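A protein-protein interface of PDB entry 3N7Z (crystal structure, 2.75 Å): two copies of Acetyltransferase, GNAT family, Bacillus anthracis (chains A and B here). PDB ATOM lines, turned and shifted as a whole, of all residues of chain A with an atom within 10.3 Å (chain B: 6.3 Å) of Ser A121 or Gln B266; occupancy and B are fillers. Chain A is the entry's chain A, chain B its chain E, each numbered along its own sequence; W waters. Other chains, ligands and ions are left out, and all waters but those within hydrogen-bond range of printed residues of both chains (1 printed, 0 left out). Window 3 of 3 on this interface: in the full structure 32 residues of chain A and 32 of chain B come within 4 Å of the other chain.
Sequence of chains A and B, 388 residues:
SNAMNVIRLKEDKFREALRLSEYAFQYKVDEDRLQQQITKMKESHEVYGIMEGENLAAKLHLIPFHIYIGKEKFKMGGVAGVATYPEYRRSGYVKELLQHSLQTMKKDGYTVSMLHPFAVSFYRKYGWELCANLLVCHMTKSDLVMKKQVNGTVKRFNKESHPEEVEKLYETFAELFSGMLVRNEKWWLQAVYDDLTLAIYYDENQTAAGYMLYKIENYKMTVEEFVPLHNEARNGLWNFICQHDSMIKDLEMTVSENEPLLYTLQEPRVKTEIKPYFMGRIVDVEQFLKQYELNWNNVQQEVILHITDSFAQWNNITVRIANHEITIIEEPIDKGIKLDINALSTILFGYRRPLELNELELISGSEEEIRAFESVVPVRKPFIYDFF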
ATOM      1  N   ARG A  89     -19.264  21.305 -20.527  1.00  0.00           N
ATOM      2  CA  ARG A  89     -18.737  20.005 -20.100  1.00  0.00           C
ATOM      3  C   ARG A  89     -17.988  20.036 -18.769  1.00  0.00           C
ATOM      4  O   ARG A  89     -17.949  19.034 -18.063  1.00  0.00           O
ATOM      5  CB  ARG A  89     -17.831  19.440 -21.182  1.00  0.00           C
ATOM      6  CG  ARG A  89     -17.687  17.940 -21.170  1.00  0.00           C
ATOM      7  CD  ARG A  89     -16.245  17.600 -21.456  1.00  0.00           C
ATOM      8  NE  ARG A  89     -16.088  16.357 -22.204  1.00  0.00           N
ATOM      9  CZ  ARG A  89     -14.947  15.967 -22.767  1.00  0.00           C
ATOM     10  NH1 ARG A  89     -13.855  16.721 -22.669  1.00  0.00           N
ATOM     11  NH2 ARG A  89     -14.895  14.823 -23.437  1.00  0.00           N
ATOM     12  N   LEU A  98     -27.593  11.400 -15.007  1.00  0.00           N
ATOM     13  CA  LEU A  98     -27.544   9.957 -14.958  1.00  0.00           C
ATOM     14  C   LEU A  98     -27.941   9.464 -13.573  1.00  0.00           C
ATOM     15  O   LEU A  98     -28.738   8.538 -13.443  1.00  0.00           O
ATOM     16  CB  LEU A  98     -26.148   9.481 -15.337  1.00  0.00           C
ATOM     17  CG  LEU A  98     -25.925   7.985 -15.491  1.00  0.00           C
ATOM     18  CD1 LEU A  98     -26.606   7.462 -16.746  1.00  0.00           C
ATOM     19  CD2 LEU A  98     -24.423   7.704 -15.520  1.00  0.00           C
ATOM     20  N   LEU A 115     -27.672   0.649 -22.188  1.00  0.00           N
ATOM     21  CA  LEU A 115     -27.215   1.781 -22.986  1.00  0.00           C
ATOM     22  C   LEU A 115     -26.040   1.414 -23.892  1.00  0.00           C
ATOM     23  O   LEU A 115     -25.317   0.447 -23.640  1.00  0.00           O
ATOM     24  CB  LEU A 115     -26.846   2.971 -22.090  1.00  0.00           C
ATOM     25  CG  LEU A 115     -25.762   2.842 -21.009  1.00  0.00           C
ATOM     26  CD1 LEU A 115     -24.384   3.188 -21.550  1.00  0.00           C
ATOM     27  CD2 LEU A 115     -26.081   3.743 -19.826  1.00  0.00           C
ATOM     28  N   HIS A 116     -25.872   2.203 -24.947  1.00  0.00           N
ATOM     29  CA  HIS A 116     -24.693   2.169 -25.801  1.00  0.00           C
ATOM     30  C   HIS A 116     -23.776   3.344 -25.440  1.00  0.00           C
ATOM     31  O   HIS A 116     -24.168   4.496 -25.592  1.00  0.00           O
ATOM     32  CB  HIS A 116     -25.132   2.273 -27.249  1.00  0.00           C
ATOM     33  CG  HIS A 116     -24.003   2.314 -28.220  1.00  0.00           C
ATOM     34  ND1 HIS A 116     -23.482   3.496 -28.702  1.00  0.00           N
ATOM     35  CD2 HIS A 116     -23.298   1.318 -28.805  1.00  0.00           C
ATOM     36  CE1 HIS A 116     -22.498   3.225 -29.539  1.00  0.00           C
ATOM     37  NE2 HIS A 116     -22.366   1.912 -29.621  1.00  0.00           N
ATOM     38  N   PRO A 117     -22.543   3.056 -24.977  1.00  0.00           N
ATOM     39  CA  PRO A 117     -21.682   4.078 -24.363  1.00  0.00           C
ATOM     40  C   PRO A 117     -20.832   4.906 -25.333  1.00  0.00           C
ATOM     41  O   PRO A 117     -20.277   4.372 -26.297  1.00  0.00           O
ATOM     42  CB  PRO A 117     -20.759   3.249 -23.476  1.00  0.00           C
ATOM     43  CG  PRO A 117     -20.640   1.932 -24.182  1.00  0.00           C
ATOM     44  CD  PRO A 117     -21.859   1.750 -25.056  1.00  0.00           C
ATOM     45  N   PHE A 118     -20.714   6.202 -25.064  1.00  0.00           N
ATOM     46  CA  PHE A 118     -19.776   7.032 -25.796  1.00  0.00           C
ATOM     47  C   PHE A 118     -18.389   6.680 -25.296  1.00  0.00           C
ATOM     48  O   PHE A 118     -17.407   6.790 -26.024  1.00  0.00           O
ATOM     49  CB  PHE A 118     -20.068   8.519 -25.605  1.00  0.00           C
ATOM     50  CG  PHE A 118     -20.071   8.977 -24.157  1.00  0.00           C
ATOM     51  CD1 PHE A 118     -21.270   9.135 -23.464  1.00  0.00           C
ATOM     52  CD2 PHE A 118     -18.875   9.291 -23.501  1.00  0.00           C
ATOM     53  CE1 PHE A 118     -21.276   9.580 -22.135  1.00  0.00           C
ATOM     54  CE2 PHE A 118     -18.876   9.725 -22.163  1.00  0.00           C
ATOM     55  CZ  PHE A 118     -20.080   9.875 -21.488  1.00  0.00           C
ATOM     56  N   ALA A 119     -18.330   6.250 -24.038  1.00  0.00           N
ATOM     57  CA  ALA A 119     -17.107   5.754 -23.423  1.00  0.00           C
ATOM     58  C   ALA A 119     -17.507   4.739 -22.376  1.00  0.00           C
ATOM     59  O   ALA A 119     -18.344   5.028 -21.526  1.00  0.00           O
ATOM     60  CB  ALA A 119     -16.310   6.893 -22.783  1.00  0.00           C
ATOM     61  N   VAL A 120     -16.913   3.551 -22.447  1.00  0.00           N
ATOM     62  CA  VAL A 120     -17.169   2.505 -21.463  1.00  0.00           C
ATOM     63  C   VAL A 120     -16.769   2.961 -20.050  1.00  0.00           C
ATOM     64  O   VAL A 120     -17.511   2.744 -19.082  1.00  0.00           O
ATOM     65  CB  VAL A 120     -16.450   1.201 -21.840  1.00  0.00           C
ATOM     66  CG1 VAL A 120     -16.676   0.136 -20.777  1.00  0.00           C
ATOM     67  CG2 VAL A 120     -16.932   0.703 -23.195  1.00  0.00           C
ATOM     68  N   SER A 121     -15.615   3.622 -19.948  1.00  0.00           N
ATOM     69  CA  SER A 121     -15.054   4.023 -18.660  1.00  0.00           C
ATOM     70  C   SER A 121     -16.013   4.892 -17.861  1.00  0.00           C
ATOM     71  O   SER A 121     -16.084   4.794 -16.624  1.00  0.00           O
ATOM     72  CB  SER A 121     -13.765   4.799 -18.872  1.00  0.00           C
ATOM     73  OG  SER A 121     -14.062   6.123 -19.270  1.00  0.00           O
ATOM     74  N   PHE A 122     -16.739   5.750 -18.578  1.00  0.00           N
ATOM     75  CA  PHE A 122     -17.628   6.719 -17.943  1.00  0.00           C
ATOM     76  C   PHE A 122     -18.796   6.048 -17.216  1.00  0.00           C
ATOM     77  O   PHE A 122     -19.077   6.346 -16.061  1.00  0.00           O
ATOM     78  CB  PHE A 122     -18.146   7.749 -18.955  1.00  0.00           C
ATOM     79  CG  PHE A 122     -19.020   8.791 -18.336  1.00  0.00           C
ATOM     80  CD1 PHE A 122     -18.452   9.924 -17.744  1.00  0.00           C
ATOM     81  CD2 PHE A 122     -20.405   8.620 -18.290  1.00  0.00           C
ATOM     82  CE1 PHE A 122     -19.249  10.881 -17.138  1.00  0.00           C
ATOM     83  CE2 PHE A 122     -21.211   9.568 -17.689  1.00  0.00           C
ATOM     84  CZ  PHE A 122     -20.635  10.700 -17.111  1.00  0.00           C
ATOM     85  N   TYR A 123     -19.467   5.133 -17.897  1.00  0.00           N
ATOM     86  CA  TYR A 123     -20.615   4.479 -17.311  1.00  0.00           C
ATOM     87  C   TYR A 123     -20.220   3.387 -16.336  1.00  0.00           C
ATOM     88  O   TYR A 123     -21.013   3.008 -15.477  1.00  0.00           O
ATOM     89  CB  TYR A 123     -21.484   3.912 -18.402  1.00  0.00           C
ATOM     90  CG  TYR A 123     -22.074   4.959 -19.308  1.00  0.00           C
ATOM     91  CD1 TYR A 123     -23.262   5.599 -18.973  1.00  0.00           C
ATOM     92  CD2 TYR A 123     -21.456   5.300 -20.504  1.00  0.00           C
ATOM     93  CE1 TYR A 123     -23.825   6.547 -19.804  1.00  0.00           C
ATOM     94  CE2 TYR A 123     -22.010   6.254 -21.347  1.00  0.00           C
ATOM     95  CZ  TYR A 123     -23.200   6.868 -20.991  1.00  0.00           C
ATOM     96  OH  TYR A 123     -23.771   7.803 -21.816  1.00  0.00           O
ATOM     97  N   ARG A 124     -18.995   2.883 -16.459  1.00  0.00           N
ATOM     98  CA  ARG A 124     -18.498   1.909 -15.499  1.00  0.00           C
ATOM     99  C   ARG A 124     -18.556   2.462 -14.090  1.00  0.00           C
ATOM    100  O   ARG A 124     -18.954   1.759 -13.165  1.00  0.00           O
ATOM    101  CB  ARG A 124     -17.086   1.458 -15.837  1.00  0.00           C
ATOM    102  CG  ARG A 124     -17.083   0.363 -16.857  1.00  0.00           C
ATOM    103  CD  ARG A 124     -15.753  -0.341 -16.935  1.00  0.00           C
ATOM    104  NE  ARG A 124     -15.917  -1.598 -17.659  1.00  0.00           N
ATOM    105  CZ  ARG A 124     -14.937  -2.302 -18.207  1.00  0.00           C
ATOM    106  NH1 ARG A 124     -13.681  -1.887 -18.128  1.00  0.00           N
ATOM    107  NH2 ARG A 124     -15.223  -3.434 -18.830  1.00  0.00           N
ATOM    108  N   LYS A 125     -18.197   3.734 -13.945  1.00  0.00           N
ATOM    109  CA  LYS A 125     -18.110   4.375 -12.637  1.00  0.00           C
ATOM    110  C   LYS A 125     -19.444   4.430 -11.899  1.00  0.00           C
ATOM    111  O   LYS A 125     -19.464   4.390 -10.669  1.00  0.00           O
ATOM    112  CB  LYS A 125     -17.522   5.783 -12.761  1.00  0.00           C
ATOM    113  CG  LYS A 125     -16.891   6.280 -11.475  1.00  0.00           C
ATOM    114  CD  LYS A 125     -16.901   7.803 -11.387  1.00  0.00           C
ATOM    115  CE  LYS A 125     -16.754   8.271  -9.948  1.00  0.00           C
ATOM    116  NZ  LYS A 125     -16.002   9.545  -9.915  1.00  0.00           N
ATOM    117  N   TYR A 126     -20.546   4.510 -12.649  1.00  0.00           N
ATOM    118  CA  TYR A 126     -21.882   4.691 -12.067  1.00  0.00           C
ATOM    119  C   TYR A 126     -22.707   3.405 -12.072  1.00  0.00           C
ATOM    120  O   TYR A 126     -23.933   3.442 -11.919  1.00  0.00           O
ATOM    121  CB  TYR A 126     -22.605   5.865 -12.741  1.00  0.00           C
ATOM    122  CG  TYR A 126     -21.777   7.122 -12.660  1.00  0.00           C
ATOM    123  CD1 TYR A 126     -21.834   7.958 -11.538  1.00  0.00           C
ATOM    124  CD2 TYR A 126     -20.885   7.452 -13.679  1.00  0.00           C
ATOM    125  CE1 TYR A 126     -21.036   9.108 -11.457  1.00  0.00           C
ATOM    126  CE2 TYR A 126     -20.073   8.592 -13.604  1.00  0.00           C
ATOM    127  CZ  TYR A 126     -20.150   9.415 -12.496  1.00  0.00           C
ATOM    128  OH  TYR A 126     -19.345  10.538 -12.441  1.00  0.00           O
ATOM    129  N   GLY A 127     -22.020   2.272 -12.256  1.00  0.00           N
ATOM    130  CA  GLY A 127     -22.616   0.954 -12.045  1.00  0.00           C
ATOM    131  C   GLY A 127     -22.827   0.040 -13.238  1.00  0.00           C
ATOM    132  O   GLY A 127     -22.987  -1.170 -13.054  1.00  0.00           O
ATOM    133  N   TRP A 128     -22.851   0.607 -14.448  1.00  0.00           N
ATOM    134  CA  TRP A 128     -23.012  -0.176 -15.684  1.00  0.00           C
ATOM    135  C   TRP A 128     -21.774  -0.992 -16.010  1.00  0.00           C
ATOM    136  O   TRP A 128     -20.660  -0.606 -15.670  1.00  0.00           O
ATOM    137  CB  TRP A 128     -23.315   0.720 -16.884  1.00  0.00           C
ATOM    138  CG  TRP A 128     -24.745   1.134 -16.990  1.00  0.00           C
ATOM    139  CD1 TRP A 128     -25.698   0.614 -17.834  1.00  0.00           C
ATOM    140  CD2 TRP A 128     -25.402   2.154 -16.225  1.00  0.00           C
ATOM    141  NE1 TRP A 128     -26.903   1.249 -17.633  1.00  0.00           N
ATOM    142  CE2 TRP A 128     -26.748   2.200 -16.656  1.00  0.00           C
ATOM    143  CE3 TRP A 128     -24.986   3.027 -15.215  1.00  0.00           C
ATOM    144  CZ2 TRP A 128     -27.674   3.098 -16.119  1.00  0.00           C
ATOM    145  CZ3 TRP A 128     -25.912   3.914 -14.680  1.00  0.00           C
ATOM    146  CH2 TRP A 128     -27.243   3.938 -15.134  1.00  0.00           C
ATOM    147  N   GLU A 129     -21.979  -2.122 -16.677  1.00  0.00           N
ATOM    148  CA  GLU A 129     -20.886  -2.901 -17.224  1.00  0.00           C
ATOM    149  C   GLU A 129     -21.209  -3.259 -18.647  1.00  0.00           C
ATOM    150  O   GLU A 129     -22.356  -3.118 -19.070  1.00  0.00           O
ATOM    151  CB  GLU A 129     -20.682  -4.187 -16.435  1.00  0.00           C
ATOM    152  CG  GLU A 129     -19.433  -4.203 -15.559  1.00  0.00           C
ATOM    153  CD  GLU A 129     -18.157  -3.811 -16.276  1.00  0.00           C
ATOM    154  OE1 GLU A 129     -18.055  -3.980 -17.513  1.00  0.00           O
ATOM    155  OE2 GLU A 129     -17.242  -3.337 -15.577  1.00  0.00           O
ATOM    156  N   LEU A 130     -20.203  -3.725 -19.381  1.00  0.00           N
ATOM    157  CA  LEU A 130     -20.436  -4.340 -20.682  1.00  0.00           C
ATOM    158  C   LEU A 130     -21.240  -5.604 -20.461  1.00  0.00           C
ATOM    159  O   LEU A 130     -21.018  -6.312 -19.476  1.00  0.00           O
ATOM    160  CB  LEU A 130     -19.127  -4.724 -21.342  1.00  0.00           C
ATOM    161  CG  LEU A 130     -18.197  -3.632 -21.823  1.00  0.00           C
ATOM    162  CD1 LEU A 130     -16.839  -4.268 -22.084  1.00  0.00           C
ATOM    163  CD2 LEU A 130     -18.780  -3.014 -23.082  1.00  0.00           C
ATOM    164  N   PRO A 276     -17.145  -5.761 -28.253  1.00  0.00           N
ATOM    165  CA  PRO A 276     -18.029  -5.349 -27.182  1.00  0.00           C
ATOM    166  C   PRO A 276     -18.930  -4.233 -27.684  1.00  0.00           C
ATOM    167  O   PRO A 276     -18.455  -3.297 -28.333  1.00  0.00           O
ATOM    168  CB  PRO A 276     -17.056  -4.825 -26.127  1.00  0.00           C
ATOM    169  CG  PRO A 276     -15.862  -5.658 -26.316  1.00  0.00           C
ATOM    170  CD  PRO A 276     -15.757  -5.902 -27.786  1.00  0.00           C
ATOM    171  N   MET A 279     -23.876  -1.975 -22.938  1.00  0.00           N
ATOM    172  CA  MET A 279     -23.719  -2.051 -21.488  1.00  0.00           C
ATOM    173  C   MET A 279     -25.042  -2.224 -20.782  1.00  0.00           C
ATOM    174  O   MET A 279     -26.059  -1.694 -21.214  1.00  0.00           O
ATOM    175  CB  MET A 279     -23.021  -0.808 -20.965  1.00  0.00           C
ATOM    176  CG  MET A 279     -21.617  -0.650 -21.471  1.00  0.00           C
ATOM    177  SD  MET A 279     -20.777   0.916 -20.727  1.00  0.00           S
ATOM    178  CE  MET A 279     -20.119   0.170 -19.051  1.00  0.00           C
ATOM    179  N   PHE A 311     -23.561   4.155  -6.358  1.00  0.00           N
ATOM    180  CA  PHE A 311     -24.485   5.208  -6.812  1.00  0.00           C
ATOM    181  C   PHE A 311     -25.990   4.908  -6.691  1.00  0.00           C
ATOM    182  O   PHE A 311     -26.811   5.784  -6.936  1.00  0.00           O
ATOM    183  CB  PHE A 311     -24.082   5.741  -8.197  1.00  0.00           C
ATOM    184  CG  PHE A 311     -22.939   6.730  -8.133  1.00  0.00           C
ATOM    185  CD1 PHE A 311     -23.188   8.097  -7.945  1.00  0.00           C
ATOM    186  CD2 PHE A 311     -21.607   6.292  -8.194  1.00  0.00           C
ATOM    187  CE1 PHE A 311     -22.122   9.025  -7.844  1.00  0.00           C
ATOM    188  CE2 PHE A 311     -20.536   7.208  -8.094  1.00  0.00           C
ATOM    189  CZ  PHE A 311     -20.796   8.580  -7.918  1.00  0.00           C
ATOM    190  N   ASN A 342     -21.619  -3.522 -10.992  1.00  0.00           N
ATOM    191  CA  ASN A 342     -21.015  -3.848 -12.272  1.00  0.00           C
ATOM    192  C   ASN A 342     -20.864  -5.369 -12.414  1.00  0.00           C
ATOM    193  O   ASN A 342     -21.460  -5.981 -13.310  1.00  0.00           O
ATOM    194  CB  ASN A 342     -19.644  -3.181 -12.415  1.00  0.00           C
ATOM    195  CG  ASN A 342     -19.677  -1.687 -12.151  1.00  0.00           C
ATOM    196  OD1 ASN A 342     -19.834  -1.245 -11.008  1.00  0.00           O
ATOM    197  ND2 ASN A 342     -19.487  -0.899 -13.206  1.00  0.00           N
ATOM    198  N   SER B 142      -2.889   4.967 -26.681  1.00  0.00           N
ATOM    199  CA  SER B 142      -3.892   5.429 -25.708  1.00  0.00           C
ATOM    200  C   SER B 142      -4.426   4.315 -24.794  1.00  0.00           C
ATOM    201  O   SER B 142      -4.809   4.573 -23.656  1.00  0.00           O
ATOM    202  CB  SER B 142      -5.051   6.145 -26.416  1.00  0.00           C
ATOM    203  OG  SER B 142      -5.817   5.241 -27.191  1.00  0.00           O
ATOM    204  N   ASP B 143      -4.439   3.082 -25.298  1.00  0.00           N
ATOM    205  CA  ASP B 143      -4.886   1.918 -24.529  1.00  0.00           C
ATOM    206  C   ASP B 143      -3.919   1.517 -23.400  1.00  0.00           C
ATOM    207  O   ASP B 143      -4.311   0.785 -22.486  1.00  0.00           O
ATOM    208  CB  ASP B 143      -5.158   0.725 -25.457  1.00  0.00           C
ATOM    209  CG  ASP B 143      -6.366   0.947 -26.383  1.00  0.00           C
ATOM    210  OD1 ASP B 143      -7.491   1.160 -25.874  1.00  0.00           O
ATOM    211  OD2 ASP B 143      -6.203   0.895 -27.626  1.00  0.00           O
ATOM    212  N   VAL B 145      -2.714   2.192 -20.458  1.00  0.00           N
ATOM    213  CA  VAL B 145      -2.919   2.781 -19.145  1.00  0.00           C
ATOM    214  C   VAL B 145      -2.503   1.738 -18.133  1.00  0.00           C
ATOM    215  O   VAL B 145      -2.863   0.569 -18.257  1.00  0.00           O
ATOM    216  CB  VAL B 145      -4.415   3.143 -18.935  1.00  0.00           C
ATOM    217  CG1 VAL B 145      -4.676   3.715 -17.536  1.00  0.00           C
ATOM    218  CG2 VAL B 145      -4.869   4.120 -19.996  1.00  0.00           C
ATOM    219  N   MET B 146      -1.741   2.155 -17.132  1.00  0.00           N
ATOM    220  CA  MET B 146      -1.232   1.212 -16.143  1.00  0.00           C
ATOM    221  C   MET B 146      -2.291   0.846 -15.123  1.00  0.00           C
ATOM    222  O   MET B 146      -3.157   1.664 -14.791  1.00  0.00           O
ATOM    223  CB  MET B 146      -0.013   1.780 -15.436  1.00  0.00           C
ATOM    224  CG  MET B 146       1.084   2.147 -16.387  1.00  0.00           C
ATOM    225  SD  MET B 146       2.779   1.708 -15.602  1.00  0.00           S
ATOM    226  CE  MET B 146       2.864   3.170 -14.274  1.00  0.00           C
ATOM    227  N   LYS B 147      -2.220  -0.392 -14.642  1.00  0.00           N
ATOM    228  CA  LYS B 147      -3.030  -0.821 -13.510  1.00  0.00           C
ATOM    229  C   LYS B 147      -2.246  -0.548 -12.230  1.00  0.00           C
ATOM    230  O   LYS B 147      -1.147   0.015 -12.300  1.00  0.00           O
ATOM    231  CB  LYS B 147      -3.411  -2.282 -13.673  1.00  0.00           C
ATOM    232  CG  LYS B 147      -4.334  -2.465 -14.864  1.00  0.00           C
ATOM    233  CD  LYS B 147      -4.266  -3.856 -15.464  1.00  0.00           C
ATOM    234  CE  LYS B 147      -4.967  -3.888 -16.815  1.00  0.00           C
ATOM    235  NZ  LYS B 147      -6.253  -3.117 -16.823  1.00  0.00           N
ATOM    236  N   LEU B 262      -8.564  -7.854 -22.062  1.00  0.00           N
ATOM    237  CA  LEU B 262      -9.221  -6.725 -22.730  1.00  0.00           C
ATOM    238  C   LEU B 262     -10.287  -6.068 -21.860  1.00  0.00           C
ATOM    239  O   LEU B 262     -10.384  -4.833 -21.792  1.00  0.00           O
ATOM    240  CB  LEU B 262      -9.864  -7.181 -24.031  1.00  0.00           C
ATOM    241  CG  LEU B 262      -9.030  -7.191 -25.305  1.00  0.00           C
ATOM    242  CD1 LEU B 262      -7.608  -7.680 -25.065  1.00  0.00           C
ATOM    243  CD2 LEU B 262      -9.757  -8.052 -26.342  1.00  0.00           C
ATOM    244  N   TYR B 263     -11.078  -6.908 -21.200  1.00  0.00           N
ATOM    245  CA  TYR B 263     -12.133  -6.469 -20.311  1.00  0.00           C
ATOM    246  C   TYR B 263     -11.654  -5.393 -19.322  1.00  0.00           C
ATOM    247  O   TYR B 263     -12.397  -4.473 -18.985  1.00  0.00           O
ATOM    248  CB  TYR B 263     -12.686  -7.690 -19.583  1.00  0.00           C
ATOM    249  CG  TYR B 263     -13.885  -7.424 -18.725  1.00  0.00           C
ATOM    250  CD1 TYR B 263     -15.142  -7.224 -19.288  1.00  0.00           C
ATOM    251  CD2 TYR B 263     -13.769  -7.384 -17.340  1.00  0.00           C
ATOM    252  CE1 TYR B 263     -16.246  -6.984 -18.493  1.00  0.00           C
ATOM    253  CE2 TYR B 263     -14.872  -7.139 -16.533  1.00  0.00           C
ATOM    254  CZ  TYR B 263     -16.105  -6.943 -17.113  1.00  0.00           C
ATOM    255  OH  TYR B 263     -17.195  -6.702 -16.309  1.00  0.00           O
ATOM    256  N   THR B 264     -10.402  -5.491 -18.891  1.00  0.00           N
ATOM    257  CA  THR B 264      -9.867  -4.589 -17.867  1.00  0.00           C
ATOM    258  C   THR B 264      -9.421  -3.228 -18.383  1.00  0.00           C
ATOM    259  O   THR B 264      -9.100  -2.366 -17.572  1.00  0.00           O
ATOM    260  CB  THR B 264      -8.669  -5.206 -17.092  1.00  0.00           C
ATOM    261  OG1 THR B 264      -7.602  -5.489 -18.004  1.00  0.00           O
ATOM    262  CG2 THR B 264      -9.064  -6.482 -16.384  1.00  0.00           C
ATOM    263  N   LEU B 265      -9.396  -3.033 -19.707  1.00  0.00           N
ATOM    264  CA  LEU B 265      -8.927  -1.772 -20.319  1.00  0.00           C
ATOM    265  C   LEU B 265      -9.855  -0.608 -20.025  1.00  0.00           C
ATOM    266  O   LEU B 265     -11.012  -0.825 -19.671  1.00  0.00           O
ATOM    267  CB  LEU B 265      -8.808  -1.935 -21.830  1.00  0.00           C
ATOM    268  CG  LEU B 265      -7.524  -2.475 -22.473  1.00  0.00           C
ATOM    269  CD1 LEU B 265      -6.741  -3.411 -21.576  1.00  0.00           C
ATOM    270  CD2 LEU B 265      -7.867  -3.162 -23.781  1.00  0.00           C
ATOM    271  N   GLN B 266      -9.370   0.626 -20.173  1.00  0.00           N
ATOM    272  CA  GLN B 266     -10.262   1.799 -20.029  1.00  0.00           C
ATOM    273  C   GLN B 266     -11.342   1.826 -21.120  1.00  0.00           C
ATOM    274  O   GLN B 266     -12.496   2.172 -20.860  1.00  0.00           O
ATOM    275  CB  GLN B 266      -9.490   3.113 -20.021  1.00  0.00           C
ATOM    276  CG  GLN B 266      -8.467   3.244 -18.901  1.00  0.00           C
ATOM    277  CD  GLN B 266      -9.054   3.169 -17.478  1.00  0.00           C
ATOM    278  OE1 GLN B 266      -9.882   4.003 -17.073  1.00  0.00           O
ATOM    279  NE2 GLN B 266      -8.595   2.176 -16.706  1.00  0.00           N
ATOM    280  N   GLU B 267     -10.948   1.442 -22.333  1.00  0.00           N
ATOM    281  CA  GLU B 267     -11.845   1.356 -23.472  1.00  0.00           C
ATOM    282  C   GLU B 267     -11.700  -0.027 -24.113  1.00  0.00           C
ATOM    283  O   GLU B 267     -10.923  -0.203 -25.061  1.00  0.00           O
ATOM    284  CB  GLU B 267     -11.568   2.491 -24.473  1.00  0.00           C
ATOM    285  CG  GLU B 267     -12.539   2.562 -25.664  1.00  0.00           C
ATOM    286  CD  GLU B 267     -14.011   2.455 -25.257  1.00  0.00           C
ATOM    287  OE1 GLU B 267     -14.625   1.421 -25.605  1.00  0.00           O
ATOM    288  OE2 GLU B 267     -14.538   3.384 -24.585  1.00  0.00           O
ATOM    289  N   PRO B 268     -12.460  -1.012 -23.585  1.00  0.00           N
ATOM    290  CA  PRO B 268     -12.439  -2.420 -23.988  1.00  0.00           C
ATOM    291  C   PRO B 268     -12.874  -2.690 -25.434  1.00  0.00           C
ATOM    292  O   PRO B 268     -12.588  -3.771 -25.953  1.00  0.00           O
ATOM    293  CB  PRO B 268     -13.429  -3.076 -23.014  1.00  0.00           C
ATOM    294  CG  PRO B 268     -13.545  -2.139 -21.880  1.00  0.00           C
ATOM    295  CD  PRO B 268     -13.423  -0.791 -22.491  1.00  0.00           C
HETATM  296  O   HOH W   1     -13.234   1.324 -18.246  1.00  0.00           O
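N of Val A120 lies within hydrogen-bond range of OE2 of Glu B267, at 3.2 Å. The guanidinium group (NH1) of Arg A124 sits at hydrogen-bond distance from the backbone carbonyl oxygen (O) of Leu B265, 3.3 Å away. The guanidinium group of Arg A124 lies within hydrogen-bond range of the backbone carbonyl oxygen of Tyr B263 (3.0 Å). OE1 of Glu A129 lies close to OH of Tyr B263.
O of Arg A124 lies within hydrogen-bond range of ND2 of Asn A342. The guanidinium group of Arg A124 is in salt-bridge range of the side-chain carboxylate of Glu A129.
Glu B267 touches Ala A119 (OE2 to CA, 3.7 Å). Pro B268 touches Val A120 (CD to CB, 3.7 Å). CB of Ser A121 touches O of Gln B266, 3.5 Å away. Arg A124 touches Pro B268 (NH2 to CG, 3.7 Å). Pro B268 touches Leu A130. Pro B268 touches Pro A276 (O to CG, 3.8 Å).
Pro A117 touches none of the printed residues of chain B. Printed residues of chain B within 4 Å of Ala A119: Glu B267 (3.7 Å). Printed residues of chain B within 4 Å of Val A120: Glu B267 (3.2 Å) and Pro B268 (3.7 Å). Of chain B, only Gln B266 (3.5 Å) comes within 4 Å of Ser A121. Printed residues of chain B within 4 Å of Leu A130: Pro B268. Of chain A, only Ala A119 (3.7 Å) and Val A120 (3.2 Å) come within 4 Å of Glu B267. Printed residues of chain A within 4 Å of Pro B268: Val A120 (3.7 Å), Arg A124 (3.7 Å), Leu A130 (3.7 Å) and Pro A276 (3.8 Å). The nearest residue of chain A that does not touch Gln B266 is Val A120 (4.2 Å). The nearest printed residue of chain B that does not touch Arg A124 is Thr B264 (4.5 Å).
Hydrophobic or aromatic side chains of chain B that line the printed part of chain A: Tyr B263 and Pro B268. Among the printed residues, 10 pairs touch across the chains.
No position is printed for both chains. Of the 10 pairs that touch across the chains among the printed residues, none has its exchanged pair printed and touching as well.
Water W1 lies within hydrogen-bond range of the backbone carbonyl oxygen (O) of Gln B266 (2.8 Å), the guanidinium group (NH1) of Arg A124 (3.2 Å) and the backbone carbonyl oxygen (O) of Leu B265 (3.4 Å).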
